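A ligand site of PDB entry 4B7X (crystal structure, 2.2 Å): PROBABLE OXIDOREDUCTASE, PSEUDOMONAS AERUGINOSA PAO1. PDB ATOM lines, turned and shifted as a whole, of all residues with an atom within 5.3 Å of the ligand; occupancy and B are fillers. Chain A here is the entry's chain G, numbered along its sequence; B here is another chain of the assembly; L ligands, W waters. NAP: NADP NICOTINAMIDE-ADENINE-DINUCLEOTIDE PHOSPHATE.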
ATOM      1  N   ASP A  51     -29.578 -17.536  15.383  1.00  0.00           N
ATOM      2  CA  ASP A  51     -28.951 -18.243  16.477  1.00  0.00           C
ATOM      3  C   ASP A  51     -29.948 -19.207  17.108  1.00  0.00           C
ATOM      4  O   ASP A  51     -31.159 -18.972  17.044  1.00  0.00           O
ATOM      5  CB  ASP A  51     -28.444 -17.245  17.520  1.00  0.00           C
ATOM      6  CG  ASP A  51     -27.354 -16.328  16.989  1.00  0.00           C
ATOM      7  OD1 ASP A  51     -26.317 -16.812  16.474  1.00  0.00           O
ATOM      8  OD2 ASP A  51     -27.524 -15.092  17.107  1.00  0.00           O
ATOM      9  N   PRO A  52     -29.454 -20.305  17.723  1.00  0.00           N
ATOM     10  CA  PRO A  52     -30.356 -21.193  18.441  1.00  0.00           C
ATOM     11  C   PRO A  52     -31.069 -20.488  19.594  1.00  0.00           C
ATOM     12  O   PRO A  52     -32.228 -20.789  19.863  1.00  0.00           O
ATOM     13  CB  PRO A  52     -29.415 -22.285  18.987  1.00  0.00           C
ATOM     14  CG  PRO A  52     -28.282 -22.290  18.021  1.00  0.00           C
ATOM     15  CD  PRO A  52     -28.094 -20.862  17.618  1.00  0.00           C
ATOM     16  N   ALA A  53     -30.374 -19.560  20.254  1.00  0.00           N
ATOM     17  CA  ALA A  53     -30.931 -18.801  21.383  1.00  0.00           C
ATOM     18  C   ALA A  53     -32.270 -18.117  21.055  1.00  0.00           C
ATOM     19  O   ALA A  53     -33.003 -17.748  21.979  1.00  0.00           O
ATOM     20  CB  ALA A  53     -29.931 -17.793  21.893  1.00  0.00           C
ATOM     21  N   MET A 132     -20.504 -12.971  17.916  1.00  0.00           N
ATOM     22  CA  MET A 132     -20.944 -13.536  19.175  1.00  0.00           C
ATOM     23  C   MET A 132     -20.528 -15.003  19.397  1.00  0.00           C
ATOM     24  O   MET A 132     -20.084 -15.367  20.479  1.00  0.00           O
ATOM     25  CB  MET A 132     -22.463 -13.386  19.302  1.00  0.00           C
ATOM     26  CG  MET A 132     -23.015 -13.721  20.685  1.00  0.00           C
ATOM     27  SD  MET A 132     -23.410 -15.471  20.817  1.00  0.00           S
ATOM     28  CE  MET A 132     -24.735 -15.652  19.614  1.00  0.00           C
ATOM     29  N   THR A 133     -20.713 -15.835  18.394  1.00  0.00           N
ATOM     30  CA  THR A 133     -20.397 -17.243  18.504  1.00  0.00           C
ATOM     31  C   THR A 133     -18.893 -17.468  18.639  1.00  0.00           C
ATOM     32  O   THR A 133     -18.467 -18.328  19.405  1.00  0.00           O
ATOM     33  CB  THR A 133     -20.929 -18.001  17.307  1.00  0.00           C
ATOM     34  OG1 THR A 133     -20.500 -17.327  16.136  1.00  0.00           O
ATOM     35  CG2 THR A 133     -22.467 -18.034  17.346  1.00  0.00           C
ATOM     36  N   THR A 136     -17.897 -16.405  22.160  1.00  0.00           N
ATOM     37  CA  THR A 136     -18.369 -17.443  23.080  1.00  0.00           C
ATOM     38  C   THR A 136     -17.333 -18.551  23.175  1.00  0.00           C
ATOM     39  O   THR A 136     -16.924 -18.909  24.268  1.00  0.00           O
ATOM     40  CB  THR A 136     -19.703 -18.045  22.622  1.00  0.00           C
ATOM     41  OG1 THR A 136     -20.690 -17.006  22.544  1.00  0.00           O
ATOM     42  CG2 THR A 136     -20.191 -19.090  23.589  1.00  0.00           C
ATOM     43  N   GLY A 157     -21.477 -30.438  19.533  1.00  0.00           N
ATOM     44  CA  GLY A 157     -21.815 -29.522  18.453  1.00  0.00           C
ATOM     45  C   GLY A 157     -20.599 -28.951  17.763  1.00  0.00           C
ATOM     46  O   GLY A 157     -20.586 -27.770  17.390  1.00  0.00           O
ATOM     47  N   ALA A 159     -19.237 -29.084  14.933  1.00  0.00           N
ATOM     48  CA  ALA A 159     -19.377 -28.585  13.581  1.00  0.00           C
ATOM     49  C   ALA A 159     -20.072 -27.236  13.587  1.00  0.00           C
ATOM     50  O   ALA A 159     -19.991 -26.479  12.618  1.00  0.00           O
ATOM     51  CB  ALA A 159     -20.177 -29.568  12.738  1.00  0.00           C
ATOM     52  N   GLY A 160     -20.769 -26.927  14.686  1.00  0.00           N
ATOM     53  CA  GLY A 160     -21.513 -25.677  14.809  1.00  0.00           C
ATOM     54  C   GLY A 160     -20.648 -24.440  14.965  1.00  0.00           C
ATOM     55  O   GLY A 160     -19.422 -24.507  15.070  1.00  0.00           O
ATOM     56  N   ALA A 161     -21.296 -23.283  15.001  1.00  0.00           N
ATOM     57  CA  ALA A 161     -20.579 -22.015  15.003  1.00  0.00           C
ATOM     58  C   ALA A 161     -19.670 -21.821  16.214  1.00  0.00           C
ATOM     59  O   ALA A 161     -18.526 -21.376  16.068  1.00  0.00           O
ATOM     60  CB  ALA A 161     -21.576 -20.857  14.854  1.00  0.00           C
ATOM     61  N   VAL A 162     -20.167 -22.128  17.406  1.00  0.00           N
ATOM     62  CA  VAL A 162     -19.346 -22.053  18.632  1.00  0.00           C
ATOM     63  C   VAL A 162     -18.292 -23.179  18.646  1.00  0.00           C
ATOM     64  O   VAL A 162     -17.097 -22.924  18.821  1.00  0.00           O
ATOM     65  CB  VAL A 162     -20.207 -22.122  19.917  1.00  0.00           C
ATOM     66  CG1 VAL A 162     -19.324 -22.083  21.148  1.00  0.00           C
ATOM     67  CG2 VAL A 162     -21.229 -20.984  19.991  1.00  0.00           C
ATOM     68  N   GLY A 163     -18.761 -24.420  18.477  1.00  0.00           N
ATOM     69  CA  GLY A 163     -17.912 -25.597  18.625  1.00  0.00           C
ATOM     70  C   GLY A 163     -16.744 -25.650  17.654  1.00  0.00           C
ATOM     71  O   GLY A 163     -15.642 -26.050  18.007  1.00  0.00           O
ATOM     72  N   ALA A 181     -20.249 -34.697  16.277  1.00  0.00           N
ATOM     73  CA  ALA A 181     -21.032 -34.084  15.211  1.00  0.00           C
ATOM     74  C   ALA A 181     -21.900 -35.133  14.537  1.00  0.00           C
ATOM     75  O   ALA A 181     -21.590 -36.329  14.560  1.00  0.00           O
ATOM     76  CB  ALA A 181     -20.112 -33.448  14.183  1.00  0.00           C
ATOM     77  N   GLY A 182     -22.989 -34.679  13.929  1.00  0.00           N
ATOM     78  CA  GLY A 182     -23.930 -35.570  13.244  1.00  0.00           C
ATOM     79  C   GLY A 182     -23.616 -35.725  11.779  1.00  0.00           C
ATOM     80  O   GLY A 182     -23.506 -34.734  11.047  1.00  0.00           O
ATOM     81  N   LYS A 186     -19.974 -34.156   8.158  1.00  0.00           N
ATOM     82  CA  LYS A 186     -19.560 -33.133   9.130  1.00  0.00           C
ATOM     83  C   LYS A 186     -18.333 -33.571   9.917  1.00  0.00           C
ATOM     84  O   LYS A 186     -17.402 -32.777  10.092  1.00  0.00           O
ATOM     85  CB  LYS A 186     -20.715 -32.795  10.085  1.00  0.00           C
ATOM     86  CG  LYS A 186     -21.850 -32.000   9.469  1.00  0.00           C
ATOM     87  CD  LYS A 186     -22.771 -31.442  10.560  1.00  0.00           C
ATOM     88  CE  LYS A 186     -23.771 -30.443  10.001  1.00  0.00           C
ATOM     89  NZ  LYS A 186     -24.435 -29.688  11.104  1.00  0.00           N
ATOM     90  N   TYR A 202     -22.178 -39.082  16.420  1.00  0.00           N
ATOM     91  CA  TYR A 202     -23.187 -39.447  17.416  1.00  0.00           C
ATOM     92  C   TYR A 202     -24.447 -39.996  16.746  1.00  0.00           C
ATOM     93  O   TYR A 202     -25.216 -40.713  17.376  1.00  0.00           O
ATOM     94  CB  TYR A 202     -23.508 -38.242  18.331  1.00  0.00           C
ATOM     95  CG  TYR A 202     -24.463 -37.226  17.737  1.00  0.00           C
ATOM     96  CD1 TYR A 202     -23.991 -36.140  16.996  1.00  0.00           C
ATOM     97  CD2 TYR A 202     -25.832 -37.338  17.930  1.00  0.00           C
ATOM     98  CE1 TYR A 202     -24.866 -35.206  16.449  1.00  0.00           C
ATOM     99  CE2 TYR A 202     -26.713 -36.406  17.402  1.00  0.00           C
ATOM    100  CZ  TYR A 202     -26.227 -35.349  16.651  1.00  0.00           C
ATOM    101  OH  TYR A 202     -27.110 -34.438  16.129  1.00  0.00           O
ATOM    102  N   LYS A 203     -24.646 -39.653  15.478  1.00  0.00           N
ATOM    103  CA  LYS A 203     -25.846 -40.080  14.751  1.00  0.00           C
ATOM    104  C   LYS A 203     -25.787 -41.529  14.264  1.00  0.00           C
ATOM    105  O   LYS A 203     -26.815 -42.200  14.180  1.00  0.00           O
ATOM    106  CB  LYS A 203     -26.152 -39.113  13.605  1.00  0.00           C
ATOM    107  CG  LYS A 203     -26.920 -37.878  14.071  1.00  0.00           C
ATOM    108  CD  LYS A 203     -27.366 -37.008  12.904  1.00  0.00           C
ATOM    109  CE  LYS A 203     -28.249 -35.866  13.401  1.00  0.00           C
ATOM    110  NZ  LYS A 203     -28.561 -34.868  12.332  1.00  0.00           N
ATOM    111  N   ASN A 225     -22.148 -27.863  24.137  1.00  0.00           N
ATOM    112  CA  ASN A 225     -23.154 -27.081  23.458  1.00  0.00           C
ATOM    113  C   ASN A 225     -24.518 -27.766  23.394  1.00  0.00           C
ATOM    114  O   ASN A 225     -25.515 -27.149  22.971  1.00  0.00           O
ATOM    115  CB  ASN A 225     -22.665 -26.807  22.044  1.00  0.00           C
ATOM    116  CG  ASN A 225     -21.508 -25.830  22.015  1.00  0.00           C
ATOM    117  OD1 ASN A 225     -21.636 -24.709  22.504  1.00  0.00           O
ATOM    118  ND2 ASN A 225     -20.373 -26.252  21.458  1.00  0.00           N
ATOM    119  N   VAL A 226     -24.565 -29.029  23.839  1.00  0.00           N
ATOM    120  CA  VAL A 226     -25.660 -29.940  23.471  1.00  0.00           C
ATOM    121  C   VAL A 226     -26.415 -30.506  24.663  1.00  0.00           C
ATOM    122  O   VAL A 226     -27.642 -30.600  24.630  1.00  0.00           O
ATOM    123  CB  VAL A 226     -25.128 -31.057  22.524  1.00  0.00           C
ATOM    124  CG1 VAL A 226     -26.149 -32.167  22.323  1.00  0.00           C
ATOM    125  CG2 VAL A 226     -24.727 -30.455  21.194  1.00  0.00           C
ATOM    126  N   ILE A 230     -25.284 -37.017  25.407  1.00  0.00           N
ATOM    127  CA  ILE A 230     -23.900 -36.740  25.041  1.00  0.00           C
ATOM    128  C   ILE A 230     -23.120 -36.273  26.270  1.00  0.00           C
ATOM    129  O   ILE A 230     -22.053 -36.801  26.581  1.00  0.00           O
ATOM    130  CB  ILE A 230     -23.847 -35.726  23.866  1.00  0.00           C
ATOM    131  CG1 ILE A 230     -24.483 -36.374  22.628  1.00  0.00           C
ATOM    132  CG2 ILE A 230     -22.422 -35.265  23.585  1.00  0.00           C
ATOM    133  CD1 ILE A 230     -24.166 -35.737  21.294  1.00  0.00           C
ATOM    134  N   LEU A 246     -20.243 -25.406  30.377  1.00  0.00           N
ATOM    135  CA  LEU A 246     -21.605 -25.429  29.880  1.00  0.00           C
ATOM    136  C   LEU A 246     -21.874 -24.183  29.098  1.00  0.00           C
ATOM    137  O   LEU A 246     -22.017 -23.089  29.631  1.00  0.00           O
ATOM    138  CB  LEU A 246     -22.637 -25.598  30.993  1.00  0.00           C
ATOM    139  CG  LEU A 246     -22.636 -26.919  31.756  1.00  0.00           C
ATOM    140  CD1 LEU A 246     -23.901 -26.986  32.590  1.00  0.00           C
ATOM    141  CD2 LEU A 246     -22.523 -28.136  30.830  1.00  0.00           C
ATOM    142  N   CYS A 247     -21.958 -24.354  27.803  1.00  0.00           N
ATOM    143  CA  CYS A 247     -22.180 -23.238  26.954  1.00  0.00           C
ATOM    144  C   CYS A 247     -23.634 -23.273  26.509  1.00  0.00           C
ATOM    145  O   CYS A 247     -24.287 -22.243  26.502  1.00  0.00           O
ATOM    146  CB  CYS A 247     -21.176 -23.269  25.811  1.00  0.00           C
ATOM    147  SG  CYS A 247     -21.469 -22.023  24.551  1.00  0.00           S
ATOM    148  N   GLY A 248     -24.139 -24.457  26.197  1.00  0.00           N
ATOM    149  CA  GLY A 248     -25.530 -24.618  25.819  1.00  0.00           C
ATOM    150  C   GLY A 248     -26.061 -26.032  26.019  1.00  0.00           C
ATOM    151  O   GLY A 248     -25.358 -26.907  26.569  1.00  0.00           O
ATOM    152  N   ALA A 249     -27.295 -26.247  25.591  1.00  0.00           N
ATOM    153  CA  ALA A 249     -27.945 -27.551  25.671  1.00  0.00           C
ATOM    154  C   ALA A 249     -28.977 -27.676  24.567  1.00  0.00           C
ATOM    155  O   ALA A 249     -30.138 -27.937  24.841  1.00  0.00           O
ATOM    156  CB  ALA A 249     -28.587 -27.758  27.031  1.00  0.00           C
ATOM    157  N   ILE A 250     -28.536 -27.539  23.329  1.00  0.00           N
ATOM    158  CA  ILE A 250     -29.412 -27.495  22.166  1.00  0.00           C
ATOM    159  C   ILE A 250     -30.323 -28.726  22.017  1.00  0.00           C
ATOM    160  O   ILE A 250     -31.475 -28.584  21.607  1.00  0.00           O
ATOM    161  CB  ILE A 250     -28.616 -27.196  20.873  1.00  0.00           C
ATOM    162  CG1 ILE A 250     -29.569 -26.748  19.755  1.00  0.00           C
ATOM    163  CG2 ILE A 250     -27.754 -28.382  20.468  1.00  0.00           C
ATOM    164  CD1 ILE A 250     -28.902 -25.994  18.625  1.00  0.00           C
ATOM    165  N   SER A 251     -29.841 -29.912  22.368  1.00  0.00           N
ATOM    166  CA  SER A 251     -30.673 -31.112  22.326  1.00  0.00           C
ATOM    167  C   SER A 251     -31.891 -31.037  23.261  1.00  0.00           C
ATOM    168  O   SER A 251     -32.789 -31.886  23.207  1.00  0.00           O
ATOM    169  CB  SER A 251     -29.849 -32.369  22.613  1.00  0.00           C
ATOM    170  OG  SER A 251     -29.510 -32.454  23.980  1.00  0.00           O
ATOM    171  N   TYR A 253     -33.659 -27.785  23.964  1.00  0.00           N
ATOM    172  CA  TYR A 253     -34.408 -26.529  23.798  1.00  0.00           C
ATOM    173  C   TYR A 253     -35.850 -26.701  23.325  1.00  0.00           C
ATOM    174  O   TYR A 253     -36.726 -25.915  23.697  1.00  0.00           O
ATOM    175  CB  TYR A 253     -33.673 -25.551  22.854  1.00  0.00           C
ATOM    176  CG  TYR A 253     -32.384 -24.965  23.411  1.00  0.00           C
ATOM    177  CD1 TYR A 253     -32.097 -25.022  24.774  1.00  0.00           C
ATOM    178  CD2 TYR A 253     -31.478 -24.314  22.573  1.00  0.00           C
ATOM    179  CE1 TYR A 253     -30.922 -24.489  25.294  1.00  0.00           C
ATOM    180  CE2 TYR A 253     -30.300 -23.770  23.085  1.00  0.00           C
ATOM    181  CZ  TYR A 253     -30.029 -23.867  24.436  1.00  0.00           C
ATOM    182  OH  TYR A 253     -28.877 -23.336  24.959  1.00  0.00           O
ATOM    183  N   MET A 278     -21.526 -20.305  31.474  1.00  0.00           N
ATOM    184  CA  MET A 278     -21.109 -18.940  31.119  1.00  0.00           C
ATOM    185  C   MET A 278     -22.069 -18.307  30.134  1.00  0.00           C
ATOM    186  O   MET A 278     -22.807 -18.991  29.432  1.00  0.00           O
ATOM    187  CB  MET A 278     -19.696 -18.935  30.530  1.00  0.00           C
ATOM    188  CG  MET A 278     -19.551 -19.685  29.216  1.00  0.00           C
ATOM    189  SD  MET A 278     -20.029 -18.852  27.690  1.00  0.00           S
ATOM    190  CE  MET A 278     -18.888 -17.451  27.656  1.00  0.00           C
ATOM    191  N   VAL A 279     -22.042 -16.985  30.076  1.00  0.00           N
ATOM    192  CA  VAL A 279     -22.828 -16.242  29.103  1.00  0.00           C
ATOM    193  C   VAL A 279     -21.853 -15.271  28.476  1.00  0.00           C
ATOM    194  O   VAL A 279     -21.155 -14.572  29.199  1.00  0.00           O
ATOM    195  CB  VAL A 279     -24.026 -15.509  29.793  1.00  0.00           C
ATOM    196  CG1 VAL A 279     -24.612 -14.430  28.898  1.00  0.00           C
ATOM    197  CG2 VAL A 279     -25.120 -16.515  30.160  1.00  0.00           C
ATOM    198  N   VAL A 280     -21.812 -15.258  27.145  1.00  0.00           N
ATOM    199  CA  VAL A 280     -20.805 -14.518  26.377  1.00  0.00           C
ATOM    200  C   VAL A 280     -20.789 -13.014  26.706  1.00  0.00           C
ATOM    201  O   VAL A 280     -19.732 -12.422  26.863  1.00  0.00           O
ATOM    202  CB  VAL A 280     -20.947 -14.765  24.858  1.00  0.00           C
ATOM    203  CG1 VAL A 280     -22.320 -14.314  24.364  1.00  0.00           C
ATOM    204  CG2 VAL A 280     -19.838 -14.078  24.074  1.00  0.00           C
ATOM    205  N   MET A 281     -21.976 -12.412  26.857  1.00  0.00           N
ATOM    206  CA  MET A 281     -22.055 -10.987  27.130  1.00  0.00           C
ATOM    207  C   MET A 281     -21.440 -10.596  28.472  1.00  0.00           C
ATOM    208  O   MET A 281     -21.096  -9.438  28.670  1.00  0.00           O
ATOM    209  CB  MET A 281     -23.480 -10.440  26.965  1.00  0.00           C
ATOM    210  CG  MET A 281     -24.018 -10.472  25.533  1.00  0.00           C
ATOM    211  SD  MET A 281     -22.875  -9.928  24.237  1.00  0.00           S
ATOM    212  CE  MET A 281     -22.865  -8.150  24.477  1.00  0.00           C
ATOM    213  N   LEU A 323     -32.016 -24.374  12.295  1.00  0.00           N
ATOM    214  CA  LEU A 323     -31.026 -24.390  13.373  1.00  0.00           C
ATOM    215  C   LEU A 323     -31.093 -25.588  14.324  1.00  0.00           C
ATOM    216  O   LEU A 323     -30.133 -25.846  15.077  1.00  0.00           O
ATOM    217  CB  LEU A 323     -31.066 -23.092  14.176  1.00  0.00           C
ATOM    218  CG  LEU A 323     -31.096 -21.761  13.405  1.00  0.00           C
ATOM    219  CD1 LEU A 323     -32.494 -21.160  13.460  1.00  0.00           C
ATOM    220  CD2 LEU A 323     -30.072 -20.813  14.000  1.00  0.00           C
ATOM    221  N   PHE A 324     -32.208 -26.304  14.310  1.00  0.00           N
ATOM    222  CA  PHE A 324     -32.377 -27.501  15.128  1.00  0.00           C
ATOM    223  C   PHE A 324     -32.441 -28.732  14.225  1.00  0.00           C
ATOM    224  O   PHE A 324     -32.280 -29.871  14.675  1.00  0.00           O
ATOM    225  CB  PHE A 324     -33.628 -27.391  16.005  1.00  0.00           C
ATOM    226  CG  PHE A 324     -33.737 -26.078  16.732  1.00  0.00           C
ATOM    227  CD1 PHE A 324     -33.123 -25.895  17.967  1.00  0.00           C
ATOM    228  CD2 PHE A 324     -34.468 -25.014  16.191  1.00  0.00           C
ATOM    229  CE1 PHE A 324     -33.225 -24.686  18.649  1.00  0.00           C
ATOM    230  CE2 PHE A 324     -34.564 -23.802  16.854  1.00  0.00           C
ATOM    231  CZ  PHE A 324     -33.949 -23.639  18.087  1.00  0.00           C
ATOM    232  N   GLY A 326     -30.243 -29.221  11.662  1.00  0.00           N
ATOM    233  CA  GLY A 326     -28.862 -29.604  11.399  1.00  0.00           C
ATOM    234  C   GLY A 326     -28.486 -29.341   9.944  1.00  0.00           C
ATOM    235  O   GLY A 326     -27.497 -29.881   9.446  1.00  0.00           O
ATOM    236  N   ASN A 328     -27.929 -26.155   8.546  1.00  0.00           N
ATOM    237  CA  ASN A 328     -26.934 -25.087   8.432  1.00  0.00           C
ATOM    238  C   ASN A 328     -25.514 -25.645   8.370  1.00  0.00           C
ATOM    239  O   ASN A 328     -25.075 -26.344   9.303  1.00  0.00           O
ATOM    240  CB  ASN A 328     -27.057 -24.071   9.580  1.00  0.00           C
ATOM    241  CG  ASN A 328     -26.965 -24.718  10.957  1.00  0.00           C
ATOM    242  OD1 ASN A 328     -27.742 -25.629  11.288  1.00  0.00           O
ATOM    243  ND2 ASN A 328     -26.042 -24.240  11.777  1.00  0.00           N
ATOM    244  N   GLY A 330     -22.214 -24.164   8.701  1.00  0.00           N
ATOM    245  CA  GLY A 330     -21.597 -22.915   9.114  1.00  0.00           C
ATOM    246  C   GLY A 330     -22.588 -22.066   9.872  1.00  0.00           C
ATOM    247  O   GLY A 330     -23.748 -22.468  10.061  1.00  0.00           O
ATOM    248  N   LYS A 331     -22.132 -20.903  10.324  1.00  0.00           N
ATOM    249  CA  LYS A 331     -22.963 -19.948  11.046  1.00  0.00           C
ATOM    250  C   LYS A 331     -24.041 -19.420  10.100  1.00  0.00           C
ATOM    251  O   LYS A 331     -23.731 -18.946   9.007  1.00  0.00           O
ATOM    252  CB  LYS A 331     -22.075 -18.818  11.568  1.00  0.00           C
ATOM    253  CG  LYS A 331     -22.564 -18.134  12.839  1.00  0.00           C
ATOM    254  CD  LYS A 331     -23.537 -17.005  12.533  1.00  0.00           C
ATOM    255  CE  LYS A 331     -24.173 -16.503  13.810  1.00  0.00           C
ATOM    256  NZ  LYS A 331     -25.085 -17.508  14.411  1.00  0.00           N
ATOM    257  N   LEU B 269     -25.895 -22.693  33.885  1.00  0.00           N
ATOM    258  CA  LEU B 269     -25.702 -21.852  32.711  1.00  0.00           C
ATOM    259  C   LEU B 269     -26.382 -20.474  32.886  1.00  0.00           C
ATOM    260  O   LEU B 269     -25.698 -19.428  32.875  1.00  0.00           O
ATOM    261  CB  LEU B 269     -26.231 -22.575  31.476  1.00  0.00           C
ATOM    262  CG  LEU B 269     -26.222 -21.883  30.109  1.00  0.00           C
ATOM    263  CD1 LEU B 269     -24.864 -21.298  29.770  1.00  0.00           C
ATOM    264  CD2 LEU B 269     -26.644 -22.862  29.034  1.00  0.00           C
HETATM  265  PA  NAP L   1     -24.825 -24.231  15.901  1.00  0.00           P
HETATM  266  O1A NAP L   1     -24.099 -23.422  14.692  1.00  0.00           O
HETATM  267  O2A NAP L   1     -23.915 -25.198  16.562  1.00  0.00           O
HETATM  268  O5B NAP L   1     -26.174 -24.860  15.338  1.00  0.00           O
HETATM  269  C5B NAP L   1     -26.743 -26.038  15.967  1.00  0.00           C
HETATM  270  C4B NAP L   1     -25.800 -27.270  16.033  1.00  0.00           C
HETATM  271  O4B NAP L   1     -26.162 -28.040  17.202  1.00  0.00           O
HETATM  272  C3B NAP L   1     -26.008 -28.178  14.828  1.00  0.00           C
HETATM  273  O3B NAP L   1     -24.934 -27.979  13.895  1.00  0.00           O
HETATM  274  C2B NAP L   1     -25.972 -29.605  15.406  1.00  0.00           C
HETATM  275  O2B NAP L   1     -24.767 -30.277  15.027  1.00  0.00           O
HETATM  276  C1B NAP L   1     -25.985 -29.458  16.920  1.00  0.00           C
HETATM  277  N9A NAP L   1     -27.168 -30.206  17.434  1.00  0.00           N
HETATM  278  C8A NAP L   1     -28.436 -29.800  17.344  1.00  0.00           C
HETATM  279  N7A NAP L   1     -29.243 -30.703  17.911  1.00  0.00           N
HETATM  280  C5A NAP L   1     -28.484 -31.683  18.368  1.00  0.00           C
HETATM  281  C6A NAP L   1     -28.768 -32.868  19.031  1.00  0.00           C
HETATM  282  N6A NAP L   1     -30.042 -33.159  19.326  1.00  0.00           N
HETATM  283  N1A NAP L   1     -27.751 -33.687  19.378  1.00  0.00           N
HETATM  284  C2A NAP L   1     -26.498 -33.366  19.080  1.00  0.00           C
HETATM  285  N3A NAP L   1     -26.189 -32.233  18.439  1.00  0.00           N
HETATM  286  C4A NAP L   1     -27.157 -31.379  18.073  1.00  0.00           C
HETATM  287  O3  NAP L   1     -25.274 -23.211  17.011  1.00  0.00           O
HETATM  288  PN  NAP L   1     -24.260 -22.366  17.854  1.00  0.00           P
HETATM  289  O1N NAP L   1     -24.483 -20.957  17.477  1.00  0.00           O
HETATM  290  O2N NAP L   1     -22.889 -22.932  17.752  1.00  0.00           O
HETATM  291  O5D NAP L   1     -24.803 -22.611  19.329  1.00  0.00           O
HETATM  292  C5D NAP L   1     -24.290 -23.699  20.101  1.00  0.00           C
HETATM  293  C4D NAP L   1     -24.994 -23.868  21.457  1.00  0.00           C
HETATM  294  O4D NAP L   1     -24.427 -22.947  22.423  1.00  0.00           O
HETATM  295  C3D NAP L   1     -26.503 -23.591  21.456  1.00  0.00           C
HETATM  296  O3D NAP L   1     -27.080 -24.387  22.483  1.00  0.00           O
HETATM  297  C2D NAP L   1     -26.534 -22.105  21.831  1.00  0.00           C
HETATM  298  O2D NAP L   1     -27.798 -21.699  22.363  1.00  0.00           O
HETATM  299  C1D NAP L   1     -25.472 -22.056  22.912  1.00  0.00           C
HETATM  300  N1N NAP L   1     -24.840 -20.700  22.973  1.00  0.00           N
HETATM  301  C2N NAP L   1     -24.533 -20.175  24.217  1.00  0.00           C
HETATM  302  C3N NAP L   1     -23.946 -18.928  24.321  1.00  0.00           C
HETATM  303  C7N NAP L   1     -23.604 -18.389  25.708  1.00  0.00           C
HETATM  304  O7N NAP L   1     -23.134 -17.256  25.850  1.00  0.00           O
HETATM  305  N7N NAP L   1     -23.823 -19.230  26.713  1.00  0.00           N
HETATM  306  C4N NAP L   1     -23.664 -18.186  23.173  1.00  0.00           C
HETATM  307  C5N NAP L   1     -23.965 -18.709  21.910  1.00  0.00           C
HETATM  308  C6N NAP L   1     -24.561 -19.965  21.802  1.00  0.00           C
HETATM  309  P2B NAP L   1     -24.877 -31.507  14.011  1.00  0.00           P
HETATM  310  O1X NAP L   1     -25.818 -32.556  14.788  1.00  0.00           O
HETATM  311  O2X NAP L   1     -25.727 -30.983  12.748  1.00  0.00           O
HETATM  312  O3X NAP L   1     -23.559 -32.057  13.604  1.00  0.00           O
HETATM  313  O   HOH W   1     -25.408 -20.185  14.718  1.00  0.00           O
HETATM  314  O   HOH W   2     -21.452 -25.327  18.465  1.00  0.00           O
HETATM  315  O   HOH W   3     -28.197 -35.844  21.313  1.00  0.00           O
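OH of Tyr 253 is in hydrogen-bond range of O3D of the ligand, at 3.2 Å. O2N of the ligand sits at hydrogen-bond distance from N of Val 162, 2.9 Å away. N7N of the ligand sits at hydrogen-bond distance from O of Met 278 (2.9 Å). The backbone NH (N) of Ala 161 sits at hydrogen-bond distance from an oxygen (O1A) of the ligand, at 2.8 Å. The side-chain amino group of Lys 186 lies within salt-bridge range of an oxygen (O2X) of the ligand, at 2.5 Å. An oxygen (O7N) of the ligand sits at hydrogen-bond distance from the backbone NH (N) of Val 280 (2.7 Å). OD1 of Asn 225 lies close to O4D of the ligand (3.3 Å). The backbone carbonyl oxygen of Asn 225 is in hydrogen-bond range of an oxygen (O3D) of the ligand. An oxygen (O1X) of the ligand is in hydrogen-bond range of the side-chain hydroxyl of Tyr 202, at 2.6 Å. The side-chain sulfur (SG) of Cys 247 lies close to an oxygen (O4D) of the ligand, at 3.8 Å. The backbone carbonyl oxygen (O) of Cys 247 lies within hydrogen-bond range of a nitrogen (N7N) of the ligand. The backbone NH (N) of Gly 182 lies within hydrogen-bond range of an oxygen (O3X) of the ligand.
The backbone NH (N) of Met 278 sits at hydrogen-bond distance from the backbone carbonyl oxygen (O) of Leu 246, 3.4 Å away. N of Ala 249 sits at hydrogen-bond distance from O of Asn 225. OH of Tyr 253 is in hydrogen-bond range of N of Ala 249, 3.4 Å away. The backbone carbonyl oxygen of Gly 330 is in hydrogen-bond range of the side-chain amide nitrogen of Asn 328 (3.4 Å). The backbone carbonyl oxygen (O) of Gly 326 lies within hydrogen-bond range of the side-chain amino group (NZ) of Lys 186, at 3.5 Å. The backbone NH (N) of Ile 250 lies within hydrogen-bond range of the backbone carbonyl oxygen (O) of Val 226, 3.4 Å away. The side-chain hydroxyl (OG1) of Thr 136 sits at hydrogen-bond distance from the backbone carbonyl oxygen (O) of Met 132 (2.7 Å). OG of Ser 251 lies within hydrogen-bond range of O of Val 226.
Merely in contact with the ligand: Gly 160, Thr 136, Pro 52, Ser 251, Val 279, Ile 250, Met 132, Val 226, Leu 323, Thr 133, Asn 328, Ala 181, Ala 249, Gly 326, Gly 248, Leu 269 of chain B, Ala 53 and Ile 230. Hydrophobic or aromatic side chains within 4 Å of the ligand: Pro 52, Met 132, Ala 161, Val 162, Ala 181, Tyr 202, Val 226, Ile 230, Ile 250, Tyr 253, Met 278, Val 280 and Leu 269 of chain B. Within 4 Å of the ligand: Pro 52, Ala 53, Met 132, Thr 133, Thr 136, Gly 160, Ala 161, Val 162, Ala 181, Gly 182, Lys 186, Tyr 202, Asn 225, Val 226, Ile 230, Cys 247, Gly 248, Ala 249, Ile 250, Ser 251, Tyr 253, Met 278, Val 279, Val 280, Leu 323, Gly 326, Asn 328 and Leu 269 of chain B.
Water W2 lies within hydrogen-bond range of the backbone carbonyl oxygen (O) of Gly 157 (2.8 Å), the backbone NH (N) of Gly 163 (2.8 Å), an oxygen (O2N) of the ligand (2.9 Å) and the side-chain amide nitrogen (ND2) of Asn 225 (3.3 Å). Water W1 lies within hydrogen-bond range of NZ of Lys 331 (2.7 Å) and O1N of the ligand (3.0 Å).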
